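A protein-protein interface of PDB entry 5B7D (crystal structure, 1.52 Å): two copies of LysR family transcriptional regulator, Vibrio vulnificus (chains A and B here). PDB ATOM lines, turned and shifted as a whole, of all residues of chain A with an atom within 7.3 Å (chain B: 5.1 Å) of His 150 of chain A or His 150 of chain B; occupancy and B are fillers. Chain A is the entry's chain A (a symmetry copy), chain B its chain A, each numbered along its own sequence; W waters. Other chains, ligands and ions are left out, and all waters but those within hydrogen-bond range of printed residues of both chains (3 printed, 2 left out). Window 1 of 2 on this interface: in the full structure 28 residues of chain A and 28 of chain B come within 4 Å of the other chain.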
ATOM      1  N   PRO A  24       5.159  34.672  15.179  1.00  0.00           N
ATOM      2  CA  PRO A  24       4.765  33.358  14.644  1.00  0.00           C
ATOM      3  C   PRO A  24       4.851  32.197  15.628  1.00  0.00           C
ATOM      4  O   PRO A  24       4.093  31.240  15.447  1.00  0.00           O
ATOM      5  CB  PRO A  24       5.721  33.166  13.459  1.00  0.00           C
ATOM      6  CG  PRO A  24       6.087  34.596  13.036  1.00  0.00           C
ATOM      7  CD  PRO A  24       6.220  35.301  14.369  1.00  0.00           C
ATOM      8  N   ALA A  27       1.447  33.021  17.965  1.00  0.00           N
ATOM      9  CA  ALA A  27       0.114  33.281  17.414  1.00  0.00           C
ATOM     10  C   ALA A  27      -0.714  32.025  17.167  1.00  0.00           C
ATOM     11  O   ALA A  27      -1.902  32.023  17.538  1.00  0.00           O
ATOM     12  CB  ALA A  27       0.241  34.106  16.126  1.00  0.00           C
ATOM     13  N   PRO A  28      -0.179  30.946  16.573  1.00  0.00           N
ATOM     14  CA  PRO A  28      -1.020  29.762  16.296  1.00  0.00           C
ATOM     15  C   PRO A  28      -1.568  29.115  17.551  1.00  0.00           C
ATOM     16  O   PRO A  28      -2.503  28.313  17.442  1.00  0.00           O
ATOM     17  CB  PRO A  28      -0.066  28.789  15.590  1.00  0.00           C
ATOM     18  CG  PRO A  28       1.124  29.625  15.146  1.00  0.00           C
ATOM     19  CD  PRO A  28       1.220  30.744  16.146  1.00  0.00           C
ATOM     20  N   PHE A  29      -0.964  29.370  18.714  1.00  0.00           N
ATOM     21  CA  PHE A  29      -1.232  28.599  19.919  1.00  0.00           C
ATOM     22  C   PHE A  29      -2.063  29.442  20.878  1.00  0.00           C
ATOM     23  O   PHE A  29      -3.282  29.244  20.983  1.00  0.00           O
ATOM     24  CB  PHE A  29       0.106  28.156  20.524  1.00  0.00           C
ATOM     25  CG  PHE A  29       1.063  27.616  19.483  1.00  0.00           C
ATOM     26  CD1 PHE A  29       0.704  26.503  18.740  1.00  0.00           C
ATOM     27  CD2 PHE A  29       2.275  28.235  19.220  1.00  0.00           C
ATOM     28  CE1 PHE A  29       1.544  25.997  17.743  1.00  0.00           C
ATOM     29  CE2 PHE A  29       3.136  27.720  18.233  1.00  0.00           C
ATOM     30  CZ  PHE A  29       2.760  26.593  17.495  1.00  0.00           C
ATOM     31  N   LEU A  31      -3.297  32.458  20.827  1.00  0.00           N
ATOM     32  CA  LEU A  31      -4.419  33.286  20.365  1.00  0.00           C
ATOM     33  C   LEU A  31      -5.710  32.491  20.223  1.00  0.00           C
ATOM     34  O   LEU A  31      -6.800  33.068  20.335  1.00  0.00           O
ATOM     35  CB  LEU A  31      -4.084  33.966  19.040  1.00  0.00           C
ATOM     36  CG  LEU A  31      -2.961  35.012  19.146  1.00  0.00           C
ATOM     37  CD1 LEU A  31      -2.805  35.689  17.768  1.00  0.00           C
ATOM     38  CD2 LEU A  31      -3.278  36.072  20.201  1.00  0.00           C
ATOM     39  N   CYS A  32      -5.628  31.184  19.966  1.00  0.00           N
ATOM     40  CA  CYS A  32      -6.848  30.372  19.951  1.00  0.00           C
ATOM     41  C   CYS A  32      -7.557  30.452  21.291  1.00  0.00           C
ATOM     42  O   CYS A  32      -8.792  30.598  21.356  1.00  0.00           O
ATOM     43  CB  CYS A  32      -6.517  28.909  19.644  1.00  0.00           C
ATOM     44  SG  CYS A  32      -5.812  28.554  18.033  1.00  0.00           S
ATOM     45  N   LEU A  49      -6.352  40.698  13.785  1.00  0.00           N
ATOM     46  CA  LEU A  49      -5.103  40.046  14.138  1.00  0.00           C
ATOM     47  C   LEU A  49      -4.062  40.174  13.039  1.00  0.00           C
ATOM     48  O   LEU A  49      -4.378  40.046  11.849  1.00  0.00           O
ATOM     49  CB  LEU A  49      -5.344  38.561  14.432  1.00  0.00           C
ATOM     50  CG  LEU A  49      -6.155  38.234  15.682  1.00  0.00           C
ATOM     51  CD1 LEU A  49      -6.387  36.726  15.753  1.00  0.00           C
ATOM     52  CD2 LEU A  49      -5.375  38.691  16.909  1.00  0.00           C
ATOM     53  N   GLU A  51      -0.051  38.715  12.174  1.00  0.00           N
ATOM     54  CA  GLU A  51       1.088  37.869  12.507  1.00  0.00           C
ATOM     55  C   GLU A  51       2.289  38.352  11.705  1.00  0.00           C
ATOM     56  O   GLU A  51       2.199  38.497  10.485  1.00  0.00           O
ATOM     57  CB  GLU A  51       0.797  36.389  12.197  1.00  0.00           C
ATOM     58  CG  GLU A  51       1.990  35.466  12.566  1.00  0.00           C
ATOM     59  CD  GLU A  51       1.693  33.972  12.364  1.00  0.00           C
ATOM     60  OE1 GLU A  51       2.597  33.230  11.903  1.00  0.00           O
ATOM     61  OE2 GLU A  51       0.570  33.541  12.658  1.00  0.00           O
ATOM     62  N   LEU A 119      15.670  27.914  14.178  1.00  0.00           N
ATOM     63  CA  LEU A 119      15.151  28.904  13.248  1.00  0.00           C
ATOM     64  C   LEU A 119      16.218  29.937  12.929  1.00  0.00           C
ATOM     65  O   LEU A 119      17.064  30.285  13.766  1.00  0.00           O
ATOM     66  CB  LEU A 119      13.931  29.604  13.839  1.00  0.00           C
ATOM     67  CG  LEU A 119      12.720  28.692  13.979  1.00  0.00           C
ATOM     68  CD1 LEU A 119      11.680  29.325  14.890  1.00  0.00           C
ATOM     69  CD2 LEU A 119      12.103  28.391  12.594  1.00  0.00           C
ATOM     70  N   THR A 147      12.945  27.729   8.834  1.00  0.00           N
ATOM     71  CA  THR A 147      12.229  28.947   8.495  1.00  0.00           C
ATOM     72  C   THR A 147      10.799  28.975   9.017  1.00  0.00           C
ATOM     73  O   THR A 147      10.099  29.968   8.809  1.00  0.00           O
ATOM     74  CB  THR A 147      12.273  29.158   6.975  1.00  0.00           C
ATOM     75  OG1 THR A 147      12.099  27.892   6.322  1.00  0.00           O
ATOM     76  CG2 THR A 147      13.637  29.710   6.594  1.00  0.00           C
ATOM     77  N   SER A 148      10.354  27.941   9.724  1.00  0.00           N
ATOM     78  CA  SER A 148       9.082  27.992  10.439  1.00  0.00           C
ATOM     79  C   SER A 148       9.135  26.934  11.528  1.00  0.00           C
ATOM     80  O   SER A 148       9.862  25.944  11.417  1.00  0.00           O
ATOM     81  CB  SER A 148       7.860  27.743   9.539  1.00  0.00           C
ATOM     82  OG  SER A 148       7.782  26.379   9.118  1.00  0.00           O
ATOM     83  N   LEU A 149       8.359  27.151  12.592  1.00  0.00           N
ATOM     84  CA  LEU A 149       8.378  26.184  13.680  1.00  0.00           C
ATOM     85  C   LEU A 149       7.845  24.826  13.219  1.00  0.00           C
ATOM     86  O   LEU A 149       8.367  23.782  13.617  1.00  0.00           O
ATOM     87  CB  LEU A 149       7.556  26.714  14.861  1.00  0.00           C
ATOM     88  CG  LEU A 149       7.497  25.843  16.126  1.00  0.00           C
ATOM     89  CD1 LEU A 149       8.876  25.525  16.641  1.00  0.00           C
ATOM     90  CD2 LEU A 149       6.689  26.525  17.247  1.00  0.00           C
ATOM     91  N   HIS A 150       6.823  24.823  12.363  1.00  0.00           N
ATOM     92  CA  HIS A 150       6.275  23.555  11.881  1.00  0.00           C
ATOM     93  C   HIS A 150       7.304  22.749  11.105  1.00  0.00           C
ATOM     94  O   HIS A 150       7.395  21.523  11.273  1.00  0.00           O
ATOM     95  CB  HIS A 150       5.057  23.811  10.998  1.00  0.00           C
ATOM     96  CG  HIS A 150       4.005  24.611  11.675  1.00  0.00           C
ATOM     97  ND1 HIS A 150       4.022  25.990  11.698  1.00  0.00           N
ATOM     98  CD2 HIS A 150       2.929  24.228  12.400  1.00  0.00           C
ATOM     99  CE1 HIS A 150       2.985  26.424  12.394  1.00  0.00           C
ATOM    100  NE2 HIS A 150       2.305  25.375  12.830  1.00  0.00           N
ATOM    101  N   THR A 151       8.031  23.402  10.190  1.00  0.00           N
ATOM    102  CA  THR A 151       9.004  22.644   9.393  1.00  0.00           C
ATOM    103  C   THR A 151      10.243  22.303  10.210  1.00  0.00           C
ATOM    104  O   THR A 151      10.872  21.272   9.963  1.00  0.00           O
ATOM    105  CB  THR A 151       9.382  23.399   8.107  1.00  0.00           C
ATOM    106  OG1 THR A 151       9.890  24.709   8.407  1.00  0.00           O
ATOM    107  CG2 THR A 151       8.154  23.527   7.167  1.00  0.00           C
ATOM    108  N   LEU A 152      10.592  23.123  11.207  1.00  0.00           N
ATOM    109  CA  LEU A 152      11.638  22.734  12.146  1.00  0.00           C
ATOM    110  C   LEU A 152      11.282  21.420  12.832  1.00  0.00           C
ATOM    111  O   LEU A 152      12.099  20.480  12.888  1.00  0.00           O
ATOM    112  CB  LEU A 152      11.835  23.862  13.165  1.00  0.00           C
ATOM    113  CG  LEU A 152      12.760  23.585  14.350  1.00  0.00           C
ATOM    114  CD1 LEU A 152      14.151  23.190  13.849  1.00  0.00           C
ATOM    115  CD2 LEU A 152      12.853  24.821  15.234  1.00  0.00           C
ATOM    116  N   VAL A 153      10.063  21.333  13.360  1.00  0.00           N
ATOM    117  CA  VAL A 153       9.655  20.134  14.079  1.00  0.00           C
ATOM    118  C   VAL A 153       9.585  18.951  13.133  1.00  0.00           C
ATOM    119  O   VAL A 153       9.933  17.832  13.505  1.00  0.00           O
ATOM    120  CB  VAL A 153       8.311  20.381  14.789  1.00  0.00           C
ATOM    121  CG1 VAL A 153       7.722  19.059  15.318  1.00  0.00           C
ATOM    122  CG2 VAL A 153       8.514  21.356  15.958  1.00  0.00           C
ATOM    123  N   GLN A 154       9.168  19.181  11.884  1.00  0.00           N
ATOM    124  CA  GLN A 154       9.107  18.096  10.908  1.00  0.00           C
ATOM    125  C   GLN A 154      10.501  17.534  10.608  1.00  0.00           C
ATOM    126  O   GLN A 154      10.657  16.319  10.457  1.00  0.00           O
ATOM    127  CB  GLN A 154       8.450  18.606   9.628  1.00  0.00           C
ATOM    128  CG  GLN A 154       6.931  18.640   9.673  1.00  0.00           C
ATOM    129  CD  GLN A 154       6.353  19.811   8.867  1.00  0.00           C
ATOM    130  OE1 GLN A 154       7.045  20.421   8.060  1.00  0.00           O
ATOM    131  NE2 GLN A 154       5.047  20.036   9.008  1.00  0.00           N
ATOM    132  N   MET A 155      11.522  18.401  10.509  1.00  0.00           N
ATOM    133  CA  MET A 155      12.889  17.892  10.335  1.00  0.00           C
ATOM    134  C   MET A 155      13.313  17.043  11.529  1.00  0.00           C
ATOM    135  O   MET A 155      13.940  15.991  11.356  1.00  0.00           O
ATOM    136  CB  MET A 155      13.864  19.044  10.119  1.00  0.00           C
ATOM    137  CG  MET A 155      13.682  19.717   8.748  1.00  0.00           C
ATOM    138  SD  MET A 155      15.020  20.853   8.360  1.00  0.00           S
ATOM    139  CE  MET A 155      14.627  22.276   9.408  1.00  0.00           C
ATOM    140  N   VAL A 156      12.978  17.476  12.746  1.00  0.00           N
ATOM    141  CA  VAL A 156      13.244  16.642  13.918  1.00  0.00           C
ATOM    142  C   VAL A 156      12.488  15.320  13.806  1.00  0.00           C
ATOM    143  O   VAL A 156      13.035  14.252  14.112  1.00  0.00           O
ATOM    144  CB  VAL A 156      12.888  17.398  15.213  1.00  0.00           C
ATOM    145  CG1 VAL A 156      13.017  16.450  16.432  1.00  0.00           C
ATOM    146  CG2 VAL A 156      13.833  18.588  15.428  1.00  0.00           C
ATOM    147  N   LEU A 174       1.079  20.448  18.573  1.00  0.00           N
ATOM    148  CA  LEU A 174       2.018  20.551  17.457  1.00  0.00           C
ATOM    149  C   LEU A 174       2.731  19.223  17.214  1.00  0.00           C
ATOM    150  O   LEU A 174       3.082  18.894  16.060  1.00  0.00           O
ATOM    151  CB  LEU A 174       3.013  21.686  17.723  1.00  0.00           C
ATOM    152  CG  LEU A 174       4.024  21.936  16.593  1.00  0.00           C
ATOM    153  CD1 LEU A 174       3.335  22.527  15.369  1.00  0.00           C
ATOM    154  CD2 LEU A 174       5.147  22.834  17.073  1.00  0.00           C
ATOM    155  N   GLN A 178       3.477  12.809  15.180  1.00  0.00           N
ATOM    156  CA  GLN A 178       4.821  12.902  14.623  1.00  0.00           C
ATOM    157  C   GLN A 178       5.820  12.040  15.360  1.00  0.00           C
ATOM    158  O   GLN A 178       7.013  12.068  15.019  1.00  0.00           O
ATOM    159  CB  GLN A 178       5.297  14.359  14.603  1.00  0.00           C
ATOM    160  CG  GLN A 178       4.305  15.246  13.859  1.00  0.00           C
ATOM    161  CD  GLN A 178       4.934  16.508  13.334  1.00  0.00           C
ATOM    162  OE1 GLN A 178       4.666  17.613  13.837  1.00  0.00           O
ATOM    163  NE2 GLN A 178       5.760  16.369  12.326  1.00  0.00           N
ATOM    164  N   PRO B  28       2.479  23.210   7.193  1.00  0.00           N
ATOM    165  CA  PRO B  28       2.148  22.695   8.539  1.00  0.00           C
ATOM    166  C   PRO B  28       1.359  21.404   8.505  1.00  0.00           C
ATOM    167  O   PRO B  28       1.278  20.733   9.541  1.00  0.00           O
ATOM    168  CB  PRO B  28       1.289  23.807   9.158  1.00  0.00           C
ATOM    169  CG  PRO B  28       1.527  25.040   8.301  1.00  0.00           C
ATOM    170  CD  PRO B  28       1.840  24.515   6.928  1.00  0.00           C
ATOM    171  N   PHE B  29       0.711  21.084   7.382  1.00  0.00           N
ATOM    172  CA  PHE B  29      -0.285  20.024   7.331  1.00  0.00           C
ATOM    173  C   PHE B  29       0.301  18.824   6.596  1.00  0.00           C
ATOM    174  O   PHE B  29       0.705  17.841   7.233  1.00  0.00           O
ATOM    175  CB  PHE B  29      -1.550  20.573   6.659  1.00  0.00           C
ATOM    176  CG  PHE B  29      -1.935  21.941   7.179  1.00  0.00           C
ATOM    177  CD1 PHE B  29      -2.235  22.100   8.523  1.00  0.00           C
ATOM    178  CD2 PHE B  29      -1.953  23.053   6.353  1.00  0.00           C
ATOM    179  CE1 PHE B  29      -2.558  23.354   9.048  1.00  0.00           C
ATOM    180  CE2 PHE B  29      -2.299  24.316   6.868  1.00  0.00           C
ATOM    181  CZ  PHE B  29      -2.602  24.459   8.227  1.00  0.00           C
ATOM    182  N   GLU B  51      10.182  26.795   4.448  1.00  0.00           N
ATOM    183  CA  GLU B  51       8.843  27.352   4.296  1.00  0.00           C
ATOM    184  C   GLU B  51       8.982  28.810   3.877  1.00  0.00           C
ATOM    185  O   GLU B  51       9.699  29.574   4.525  1.00  0.00           O
ATOM    186  CB  GLU B  51       8.040  27.245   5.604  1.00  0.00           C
ATOM    187  CG  GLU B  51       6.602  27.813   5.459  1.00  0.00           C
ATOM    188  CD  GLU B  51       5.741  27.628   6.719  1.00  0.00           C
ATOM    189  OE1 GLU B  51       4.963  28.552   7.064  1.00  0.00           O
ATOM    190  OE2 GLU B  51       5.839  26.573   7.360  1.00  0.00           O
ATOM    191  N   SER B 148      -1.738  35.372   8.280  1.00  0.00           N
ATOM    192  CA  SER B 148      -1.407  33.957   8.423  1.00  0.00           C
ATOM    193  C   SER B 148      -2.718  33.192   8.481  1.00  0.00           C
ATOM    194  O   SER B 148      -3.753  33.735   8.874  1.00  0.00           O
ATOM    195  CB  SER B 148      -0.572  33.645   9.677  1.00  0.00           C
ATOM    196  OG  SER B 148      -1.344  33.778  10.872  1.00  0.00           O
ATOM    197  N   LEU B 149      -2.670  31.919   8.082  1.00  0.00           N
ATOM    198  CA  LEU B 149      -3.897  31.135   8.096  1.00  0.00           C
ATOM    199  C   LEU B 149      -4.421  30.960   9.523  1.00  0.00           C
ATOM    200  O   LEU B 149      -5.632  31.005   9.752  1.00  0.00           O
ATOM    201  CB  LEU B 149      -3.649  29.772   7.440  1.00  0.00           C
ATOM    202  CG  LEU B 149      -4.849  28.818   7.323  1.00  0.00           C
ATOM    203  CD1 LEU B 149      -6.000  29.466   6.601  1.00  0.00           C
ATOM    204  CD2 LEU B 149      -4.469  27.516   6.593  1.00  0.00           C
ATOM    205  N   HIS B 150      -3.524  30.782  10.493  1.00  0.00           N
ATOM    206  CA  HIS B 150      -3.965  30.616  11.877  1.00  0.00           C
ATOM    207  C   HIS B 150      -4.705  31.840  12.389  1.00  0.00           C
ATOM    208  O   HIS B 150      -5.731  31.710  13.074  1.00  0.00           O
ATOM    209  CB  HIS B 150      -2.768  30.329  12.779  1.00  0.00           C
ATOM    210  CG  HIS B 150      -1.975  29.153  12.339  1.00  0.00           C
ATOM    211  ND1 HIS B 150      -0.978  29.244  11.389  1.00  0.00           N
ATOM    212  CD2 HIS B 150      -2.066  27.847  12.676  1.00  0.00           C
ATOM    213  CE1 HIS B 150      -0.471  28.042  11.178  1.00  0.00           C
ATOM    214  NE2 HIS B 150      -1.112  27.176  11.947  1.00  0.00           N
ATOM    215  N   THR B 151      -4.158  33.036  12.141  1.00  0.00           N
ATOM    216  CA  THR B 151      -4.824  34.237  12.659  1.00  0.00           C
ATOM    217  C   THR B 151      -6.064  34.578  11.842  1.00  0.00           C
ATOM    218  O   THR B 151      -7.019  35.137  12.387  1.00  0.00           O
ATOM    219  CB  THR B 151      -3.858  35.432  12.717  1.00  0.00           C
ATOM    220  OG1 THR B 151      -3.281  35.695  11.428  1.00  0.00           O
ATOM    221  CG2 THR B 151      -2.724  35.168  13.743  1.00  0.00           C
ATOM    222  N   LEU B 152      -6.094  34.220  10.555  1.00  0.00           N
ATOM    223  CA  LEU B 152      -7.330  34.334   9.789  1.00  0.00           C
ATOM    224  C   LEU B 152      -8.442  33.520  10.442  1.00  0.00           C
ATOM    225  O   LEU B 152      -9.562  34.019  10.663  1.00  0.00           O
ATOM    226  CB  LEU B 152      -7.068  33.871   8.351  1.00  0.00           C
ATOM    227  CG  LEU B 152      -8.277  33.736   7.426  1.00  0.00           C
ATOM    228  CD1 LEU B 152      -9.020  35.070   7.334  1.00  0.00           C
ATOM    229  CD2 LEU B 152      -7.822  33.296   6.041  1.00  0.00           C
ATOM    230  N   VAL B 153      -8.152  32.260  10.761  1.00  0.00           N
ATOM    231  CA  VAL B 153      -9.168  31.393  11.341  1.00  0.00           C
ATOM    232  C   VAL B 153      -9.567  31.897  12.715  1.00  0.00           C
ATOM    233  O   VAL B 153     -10.735  31.827  13.092  1.00  0.00           O
ATOM    234  CB  VAL B 153      -8.654  29.943  11.389  1.00  0.00           C
ATOM    235  CG1 VAL B 153      -9.584  29.063  12.247  1.00  0.00           C
ATOM    236  CG2 VAL B 153      -8.578  29.373   9.965  1.00  0.00           C
ATOM    237  N   GLN B 154      -8.613  32.446  13.474  1.00  0.00           N
ATOM    238  CA  GLN B 154      -8.930  32.983  14.796  1.00  0.00           C
ATOM    239  C   GLN B 154      -9.890  34.173  14.700  1.00  0.00           C
ATOM    240  O   GLN B 154     -10.792  34.306  15.531  1.00  0.00           O
ATOM    241  CB  GLN B 154      -7.637  33.394  15.496  1.00  0.00           C
ATOM    242  CG  GLN B 154      -6.886  32.247  16.151  1.00  0.00           C
ATOM    243  CD  GLN B 154      -5.364  32.443  16.097  1.00  0.00           C
ATOM    244  OE1 GLN B 154      -4.881  33.538  15.832  1.00  0.00           O
ATOM    245  NE2 GLN B 154      -4.623  31.401  16.469  1.00  0.00           N
ATOM    246  N   LEU B 174      -6.804  22.072  12.515  1.00  0.00           N
ATOM    247  CA  LEU B 174      -6.673  23.523  12.655  1.00  0.00           C
ATOM    248  C   LEU B 174      -7.889  24.121  13.357  1.00  0.00           C
ATOM    249  O   LEU B 174      -7.768  25.133  14.082  1.00  0.00           O
ATOM    250  CB  LEU B 174      -6.448  24.155  11.277  1.00  0.00           C
ATOM    251  CG  LEU B 174      -6.238  25.677  11.291  1.00  0.00           C
ATOM    252  CD1 LEU B 174      -4.895  26.032  11.919  1.00  0.00           C
ATOM    253  CD2 LEU B 174      -6.350  26.244   9.891  1.00  0.00           C
HETATM  254  O   HOH W   1       4.360  26.476   9.306  1.00  0.00           O
HETATM  255  O   HOH W   2      -4.258  37.873  10.188  1.00  0.00           O
HETATM  256  O   HOH W   3       0.323  31.136  12.287  1.00  0.00           O
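The side-chain amide nitrogen (NE2) of Gln 154 of chain B lies within hydrogen-bond range of the backbone carbonyl oxygen (O) of Ala 27 of chain A (3.0 Å). NE2 of Gln 154 of chain B is in hydrogen-bond range of SG of Cys 32 of chain A (3.5 Å). The side-chain hydroxyl of Thr 147 of chain A lies within hydrogen-bond range of the backbone NH of Glu 51 of chain B (2.9 Å). The side-chain carboxylate (OE2) of Glu 51 of chain B sits at hydrogen-bond distance from the side-chain hydroxyl (OG) of Ser 148 of chain A (2.6 Å). OE2 of Glu 51 of chain A is in hydrogen-bond range of OG of Ser 148 of chain B, at 2.6 Å.
OE1 of Gln 154 of chain A lies close to O of His 150 of chain A, at 3.4 Å. The side-chain hydroxyl of Ser 148 of chain B lies within hydrogen-bond range of the side-chain hydroxyl of Thr 151 of chain B. The side-chain hydroxyl (OG) of Ser 148 of chain A lies within hydrogen-bond range of the side-chain hydroxyl (OG1) of Thr 151 of chain A, at 2.8 Å. The backbone carbonyl oxygen of Pro 28 of chain A lies within hydrogen-bond range of the side-chain sulfur of Cys 32 of chain A (3.4 Å). O of His 150 of chain B lies close to OE1 of Gln 154 of chain B.
Among the printed residues, merely in contact across the chains: Leu 31 of chain A with Gln 154 of chain B, Leu 49 of chain A with Gln 154 of chain B, His 150 of chain A with Pro 28 of chain B, Pro 28 of chain A with His 150 of chain B, Leu 49 of chain A with Thr 151 of chain B, Thr 151 of chain A with Glu 51 of chain B, Glu 51 of chain A with Thr 151 of chain B, Gln 154 of chain A with Pro 28 of chain B, Pro 28 of chain A with Gln 154 of chain B, Ala 27 of chain A with Thr 151 of chain B and His 150 of chain A with His 150 of chain B.
His 150 of chain A touches just these residues of chain B: Pro 28 and His 150. His 150 of chain B touches two residues of chain A. Printed residues of chain B within 4 Å of Cys 32 of chain A: Gln 154. Printed residues of chain B within 4 Å of Pro 28 of chain A: His 150 and Gln 154. Of the printed residues of chain A, Thr 151 of chain B touches Ala 27, Leu 49 and Glu 51. Printed residues of chain B within 4 Å of Leu 49 of chain A: Thr 151 (3.8 Å) and Gln 154 (3.5 Å). Of the printed residues of chain A, Gln 154 of chain B touches Ala 27 (3.0 Å), Pro 28 (3.9 Å), Leu 31 (3.3 Å), Cys 32 (3.5 Å) and Leu 49 (3.5 Å). The nearest residue of chain A that does not touch His 150 of chain B is Glu 51 of chain A (4.6 Å).
Of the 21 printed residues of chain A, 11 touch a printed residue of chain B. Hydrophobic or aromatic side chains of chain A within 4 Å of the printed part of chain B: Ala 27, Pro 28, Leu 31, Leu 49 and His 150. Along chain A the printed residues that touch a printed residue of chain B span positions 27 to 154. Of the 11 printed residues of chain B, 6 touch a printed residue of chain A. Printed residues of chain B that touch a printed residue of chain A: Pro 28, Glu 51, Ser 148, His 150, Thr 151 and Gln 154. Among the printed residues, 16 pairs touch across the chains. Among the printed residues, no Asp or Glu carboxylate lies within 4 Å of a Lys or Arg side-chain nitrogen of the other chain.
Pro 28 of chain A touches Gln 154 of chain B, and with the chains exchanged Gln 154 of chain A touches Pro 28 of chain B. Glu 51 of chain A touches Ser 148 of chain B, and with the chains exchanged Ser 148 of chain A touches Glu 51 of chain B. Glu 51 of chain A touches Thr 151 of chain B, and with the chains exchanged Thr 151 of chain A touches Glu 51 of chain B. His 150 of chain A touches its own counterpart, His 150 of chain B. Of the 16 pairs that touch across the chains among the printed residues, 9 have their exchanged pair printed and touching as well.
Water W1 lies within hydrogen-bond range of OE2 of Glu 51 of chain B (2.4 Å), ND1 of His 150 of chain A (2.5 Å) and OG of Ser 148 of chain A (3.4 Å). Water W3 lies within hydrogen-bond range of the side-chain carboxylate (OE2) of Glu 51 of chain A (2.4 Å), a ring nitrogen (ND1) of His 150 of chain B (2.5 Å) and the side-chain hydroxyl (OG) of Ser 148 of chain B (3.4 Å). Water W2 bridges OG1 of Thr 151 of chain B (2.7 Å) and O of Leu 49 of chain A (2.7 Å).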
